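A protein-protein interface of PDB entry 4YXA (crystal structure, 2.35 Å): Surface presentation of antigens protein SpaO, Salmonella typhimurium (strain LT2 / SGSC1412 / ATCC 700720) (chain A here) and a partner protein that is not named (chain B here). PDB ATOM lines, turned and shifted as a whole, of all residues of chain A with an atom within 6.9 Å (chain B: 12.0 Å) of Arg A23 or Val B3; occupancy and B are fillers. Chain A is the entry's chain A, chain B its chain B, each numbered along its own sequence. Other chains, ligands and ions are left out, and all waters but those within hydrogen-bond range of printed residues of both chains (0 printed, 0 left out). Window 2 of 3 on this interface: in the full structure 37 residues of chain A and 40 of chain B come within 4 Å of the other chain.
Among the printed residues, merely in contact across the chains: Asp A20 with Asp B4 (3.0 Å), Thr A21 with Asp B4 (3.3 Å), Thr A21 with Leu B7 (3.5 Å), Leu A26 with Trp B68 (3.5 Å), Gln A22 with Val B5 (3.5 Å), Leu A26 with Leu B49 (3.5 Å), Gln A22 with Val B3 (3.5 Å), Gln A22 with Asp B4 (3.6 Å) and Arg A23 with Val B5 (3.8 Å).
The side-chain carboxylate (OD1) of Asp A20 is in hydrogen-bond range of the backbone NH (N) of Val B5 (2.9 Å). The backbone NH of Lys B6 lies within hydrogen-bond range of the side-chain carboxylate of Asp A20 (3.4 Å). The backbone carbonyl oxygen (O) of Val B5 is in hydrogen-bond range of the backbone NH (N) of Thr A21 (2.8 Å). The guanidinium group of Arg A23 lies close to the backbone NH of Val B3, 3.0 Å away.
The backbone carbonyl oxygen (O) of Gln A22 lies within hydrogen-bond range of the side-chain hydroxyl (OG) of Ser A24, at 3.4 Å. The backbone carbonyl oxygen (O) of Leu B49 sits at hydrogen-bond distance from the backbone NH (N) of Leu B69.
Among the printed residues, 13 pairs touch across the chains. Among the printed residues, no Asp or Glu carboxylate lies within 4 Å of a Lys or Arg side-chain nitrogen of the other chain.
Of chain B, only Asp B4 (3.3 Å), Val B5 (2.8 Å) and Leu B7 (3.5 Å) come within 4 Å of Thr A21. Gln A22 touches just these residues of chain B: Val B3 (3.5 Å), Asp B4 (3.6 Å) and Val B5 (3.5 Å). Of the printed residues of chain B, Arg A23 touches Val B3 and Val B5. No residue of chain B comes within 4 Å of Leu A25. No residue of chain B comes within 4 Å of Gly A27. Printed residues of chain A within 4 Å of Leu B7: Thr A21. Printed residues of chain A within 4 Å of Trp B68: Leu A26 (3.5 Å). The nearest printed residue of chain A that does not touch Leu B7 is Asp A20 (4.4 Å).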
ATOM      1  N   ASP A  20       5.851  -9.646  -5.256  1.00  0.00           N
ATOM      2  CA  ASP A  20       6.077 -10.104  -3.897  1.00  0.00           C
ATOM      3  C   ASP A  20       5.340  -9.232  -2.897  1.00  0.00           C
ATOM      4  O   ASP A  20       5.891  -8.310  -2.321  1.00  0.00           O
ATOM      5  CB  ASP A  20       7.564 -10.145  -3.581  1.00  0.00           C
ATOM      6  CG  ASP A  20       7.836 -10.636  -2.176  1.00  0.00           C
ATOM      7  OD1 ASP A  20       7.447 -11.787  -1.864  1.00  0.00           O
ATOM      8  OD2 ASP A  20       8.449  -9.873  -1.396  1.00  0.00           O
ATOM      9  N   THR A  21       4.071  -9.548  -2.700  1.00  0.00           N
ATOM     10  CA  THR A  21       3.240  -8.833  -1.745  1.00  0.00           C
ATOM     11  C   THR A  21       3.609  -9.219  -0.321  1.00  0.00           C
ATOM     12  O   THR A  21       4.673  -9.807  -0.091  1.00  0.00           O
ATOM     13  CB  THR A  21       1.742  -9.124  -1.985  1.00  0.00           C
ATOM     14  OG1 THR A  21       0.955  -8.481  -0.975  1.00  0.00           O
ATOM     15  CG2 THR A  21       1.483 -10.614  -1.938  1.00  0.00           C
ATOM     16  N   GLN A  22       2.737  -8.894   0.636  1.00  0.00           N
ATOM     17  CA  GLN A  22       2.970  -9.331   2.004  1.00  0.00           C
ATOM     18  C   GLN A  22       1.755  -9.238   2.930  1.00  0.00           C
ATOM     19  O   GLN A  22       1.095  -8.196   3.058  1.00  0.00           O
ATOM     20  CB  GLN A  22       4.166  -8.568   2.585  1.00  0.00           C
ATOM     21  CG  GLN A  22       3.890  -7.460   3.559  1.00  0.00           C
ATOM     22  CD  GLN A  22       5.184  -6.880   4.090  1.00  0.00           C
ATOM     23  OE1 GLN A  22       6.250  -7.490   3.955  1.00  0.00           O
ATOM     24  NE2 GLN A  22       5.102  -5.705   4.701  1.00  0.00           N
ATOM     25  N   ARG A  23       1.455 -10.404   3.502  1.00  0.00           N
ATOM     26  CA  ARG A  23       0.558 -10.625   4.636  1.00  0.00           C
ATOM     27  C   ARG A  23      -0.823  -9.971   4.647  1.00  0.00           C
ATOM     28  O   ARG A  23      -1.841 -10.644   4.544  1.00  0.00           O
ATOM     29  CB  ARG A  23       1.295 -10.229   5.942  1.00  0.00           C
ATOM     30  CG  ARG A  23       1.639  -8.742   6.141  1.00  0.00           C
ATOM     31  CD  ARG A  23       1.981  -8.355   7.610  1.00  0.00           C
ATOM     32  NE  ARG A  23       3.290  -8.789   8.065  1.00  0.00           N
ATOM     33  CZ  ARG A  23       3.621  -8.778   9.353  1.00  0.00           C
ATOM     34  NH1 ARG A  23       2.732  -8.402  10.277  1.00  0.00           N
ATOM     35  NH2 ARG A  23       4.824  -9.157   9.739  1.00  0.00           N
ATOM     36  N   SER A  24      -0.840  -8.657   4.782  1.00  0.00           N
ATOM     37  CA  SER A  24      -2.000  -7.938   5.260  1.00  0.00           C
ATOM     38  C   SER A  24      -2.919  -7.598   4.110  1.00  0.00           C
ATOM     39  O   SER A  24      -4.149  -7.605   4.261  1.00  0.00           O
ATOM     40  CB  SER A  24      -1.547  -6.677   5.985  1.00  0.00           C
ATOM     41  OG  SER A  24      -0.355  -6.200   5.369  1.00  0.00           O
ATOM     42  N   LEU A  25      -2.312  -7.345   2.949  1.00  0.00           N
ATOM     43  CA  LEU A  25      -3.075  -6.916   1.787  1.00  0.00           C
ATOM     44  C   LEU A  25      -4.079  -7.987   1.460  1.00  0.00           C
ATOM     45  O   LEU A  25      -5.272  -7.711   1.450  1.00  0.00           O
ATOM     46  CB  LEU A  25      -2.178  -6.600   0.585  1.00  0.00           C
ATOM     47  CG  LEU A  25      -0.850  -5.909   0.894  1.00  0.00           C
ATOM     48  CD1 LEU A  25       0.022  -5.741  -0.321  1.00  0.00           C
ATOM     49  CD2 LEU A  25      -1.195  -4.583   1.502  1.00  0.00           C
ATOM     50  N   LEU A  26      -3.617  -9.209   1.233  1.00  0.00           N
ATOM     51  CA  LEU A  26      -4.548 -10.315   1.268  1.00  0.00           C
ATOM     52  C   LEU A  26      -5.038 -10.379   2.696  1.00  0.00           C
ATOM     53  O   LEU A  26      -4.243 -10.488   3.616  1.00  0.00           O
ATOM     54  CB  LEU A  26      -3.896 -11.626   0.867  1.00  0.00           C
ATOM     55  CG  LEU A  26      -3.087 -11.742  -0.420  1.00  0.00           C
ATOM     56  CD1 LEU A  26      -1.600 -11.746  -0.126  1.00  0.00           C
ATOM     57  CD2 LEU A  26      -3.497 -13.019  -1.121  1.00  0.00           C
ATOM     58  N   GLY A  27      -6.341 -10.279   2.889  1.00  0.00           N
ATOM     59  CA  GLY A  27      -7.258 -10.095   1.794  1.00  0.00           C
ATOM     60  C   GLY A  27      -8.049  -8.830   2.029  1.00  0.00           C
ATOM     61  O   GLY A  27      -9.168  -8.870   2.538  1.00  0.00           O
ATOM     62  N   VAL B   3       4.886 -10.531   6.281  1.00  0.00           N
ATOM     63  CA  VAL B   3       6.149 -10.682   5.503  1.00  0.00           C
ATOM     64  C   VAL B   3       5.998 -11.258   4.039  1.00  0.00           C
ATOM     65  O   VAL B   3       5.052 -12.014   3.730  1.00  0.00           O
ATOM     66  CB  VAL B   3       7.110 -11.553   6.275  1.00  0.00           C
ATOM     67  CG1 VAL B   3       8.494 -11.460   5.755  1.00  0.00           C
ATOM     68  CG2 VAL B   3       7.132 -11.028   7.686  1.00  0.00           C
ATOM     69  N   ASP B   4       6.941 -10.881   3.159  1.00  0.00           N
ATOM     70  CA  ASP B   4       7.003 -11.252   1.727  1.00  0.00           C
ATOM     71  C   ASP B   4       6.312 -12.561   1.336  1.00  0.00           C
ATOM     72  O   ASP B   4       6.446 -13.600   1.992  1.00  0.00           O
ATOM     73  CB  ASP B   4       8.487 -11.287   1.255  1.00  0.00           C
ATOM     74  CG  ASP B   4       9.347 -12.283   2.031  1.00  0.00           C
ATOM     75  OD1 ASP B   4       8.807 -12.957   2.925  1.00  0.00           O
ATOM     76  OD2 ASP B   4      10.569 -12.361   1.771  1.00  0.00           O
ATOM     77  N   VAL B   5       5.566 -12.478   0.244  1.00  0.00           N
ATOM     78  CA  VAL B   5       4.871 -13.617  -0.322  1.00  0.00           C
ATOM     79  C   VAL B   5       4.688 -13.338  -1.808  1.00  0.00           C
ATOM     80  O   VAL B   5       4.141 -12.306  -2.208  1.00  0.00           O
ATOM     81  CB  VAL B   5       3.519 -13.882   0.378  1.00  0.00           C
ATOM     82  CG1 VAL B   5       2.836 -12.582   0.719  1.00  0.00           C
ATOM     83  CG2 VAL B   5       2.616 -14.740  -0.498  1.00  0.00           C
ATOM     84  N   LYS B   6       5.198 -14.255  -2.621  1.00  0.00           N
ATOM     85  CA  LYS B   6       5.353 -14.032  -4.048  1.00  0.00           C
ATOM     86  C   LYS B   6       4.100 -14.353  -4.829  1.00  0.00           C
ATOM     87  O   LYS B   6       3.847 -15.520  -5.118  1.00  0.00           O
ATOM     88  CB  LYS B   6       6.509 -14.872  -4.574  1.00  0.00           C
ATOM     89  CG  LYS B   6       6.679 -14.819  -6.058  1.00  0.00           C
ATOM     90  CD  LYS B   6       8.111 -15.094  -6.437  1.00  0.00           C
ATOM     91  CE  LYS B   6       8.884 -13.795  -6.575  1.00  0.00           C
ATOM     92  NZ  LYS B   6      10.362 -14.025  -6.576  1.00  0.00           N
ATOM     93  N   LEU B   7       3.313 -13.322  -5.154  1.00  0.00           N
ATOM     94  CA  LEU B   7       2.206 -13.462  -6.102  1.00  0.00           C
ATOM     95  C   LEU B   7       2.760 -13.742  -7.481  1.00  0.00           C
ATOM     96  O   LEU B   7       3.663 -13.047  -7.928  1.00  0.00           O
ATOM     97  CB  LEU B   7       1.344 -12.204  -6.177  1.00  0.00           C
ATOM     98  CG  LEU B   7       0.453 -11.731  -5.042  1.00  0.00           C
ATOM     99  CD1 LEU B   7      -0.011 -10.336  -5.381  1.00  0.00           C
ATOM    100  CD2 LEU B   7      -0.735 -12.653  -4.807  1.00  0.00           C
ATOM    101  N   ALA B  44      -0.076 -17.963  -5.532  1.00  0.00           N
ATOM    102  CA  ALA B  44       0.888 -17.583  -4.505  1.00  0.00           C
ATOM    103  C   ALA B  44       1.894 -18.676  -4.236  1.00  0.00           C
ATOM    104  O   ALA B  44       3.090 -18.497  -4.474  1.00  0.00           O
ATOM    105  CB  ALA B  44       0.181 -17.216  -3.230  1.00  0.00           C
ATOM    106  N   ASN B  45       1.412 -19.804  -3.728  1.00  0.00           N
ATOM    107  CA  ASN B  45       2.314 -20.874  -3.328  1.00  0.00           C
ATOM    108  C   ASN B  45       2.119 -22.116  -4.164  1.00  0.00           C
ATOM    109  O   ASN B  45       2.359 -23.224  -3.694  1.00  0.00           O
ATOM    110  CB  ASN B  45       2.121 -21.219  -1.849  1.00  0.00           C
ATOM    111  CG  ASN B  45       2.797 -20.232  -0.937  1.00  0.00           C
ATOM    112  OD1 ASN B  45       4.023 -20.143  -0.926  1.00  0.00           O
ATOM    113  ND2 ASN B  45       2.007 -19.491  -0.156  1.00  0.00           N
ATOM    114  N   LEU B  49      -5.345 -18.076  -6.122  1.00  0.00           N
ATOM    115  CA  LEU B  49      -6.057 -17.059  -5.342  1.00  0.00           C
ATOM    116  C   LEU B  49      -7.197 -16.435  -6.103  1.00  0.00           C
ATOM    117  O   LEU B  49      -8.293 -16.253  -5.588  1.00  0.00           O
ATOM    118  CB  LEU B  49      -5.096 -15.969  -4.912  1.00  0.00           C
ATOM    119  CG  LEU B  49      -3.913 -16.549  -4.150  1.00  0.00           C
ATOM    120  CD1 LEU B  49      -2.999 -15.447  -3.653  1.00  0.00           C
ATOM    121  CD2 LEU B  49      -4.427 -17.388  -3.001  1.00  0.00           C
ATOM    122  N   TRP B  68     -11.786 -13.705  -7.020  1.00  0.00           N
ATOM    123  CA  TRP B  68     -10.772 -13.787  -5.966  1.00  0.00           C
ATOM    124  C   TRP B  68     -11.176 -14.686  -4.801  1.00  0.00           C
ATOM    125  O   TRP B  68     -12.149 -14.410  -4.110  1.00  0.00           O
ATOM    126  CB  TRP B  68     -10.456 -12.383  -5.435  1.00  0.00           C
ATOM    127  CG  TRP B  68      -9.272 -12.343  -4.515  1.00  0.00           C
ATOM    128  CD1 TRP B  68      -9.292 -12.216  -3.158  1.00  0.00           C
ATOM    129  CD2 TRP B  68      -7.876 -12.428  -4.874  1.00  0.00           C
ATOM    130  NE1 TRP B  68      -8.016 -12.222  -2.653  1.00  0.00           N
ATOM    131  CE2 TRP B  68      -7.133 -12.349  -3.691  1.00  0.00           C
ATOM    132  CE3 TRP B  68      -7.207 -12.570  -6.099  1.00  0.00           C
ATOM    133  CZ2 TRP B  68      -5.746 -12.404  -3.683  1.00  0.00           C
ATOM    134  CZ3 TRP B  68      -5.833 -12.628  -6.083  1.00  0.00           C
ATOM    135  CH2 TRP B  68      -5.117 -12.544  -4.892  1.00  0.00           C
ATOM    136  N   LEU B  69     -10.421 -15.754  -4.586  1.00  0.00           N
ATOM    137  CA  LEU B  69     -10.637 -16.639  -3.442  1.00  0.00           C
ATOM    138  C   LEU B  69     -12.039 -17.216  -3.383  1.00  0.00           C
ATOM    139  O   LEU B  69     -12.486 -17.840  -4.330  1.00  0.00           O
ATOM    140  CB  LEU B  69     -10.346 -15.904  -2.136  1.00  0.00           C
ATOM    141  CG  LEU B  69      -8.915 -15.403  -1.984  1.00  0.00           C
ATOM    142  CD1 LEU B  69      -8.710 -14.777  -0.623  1.00  0.00           C
ATOM    143  CD2 LEU B  69      -7.935 -16.529  -2.208  1.00  0.00           C
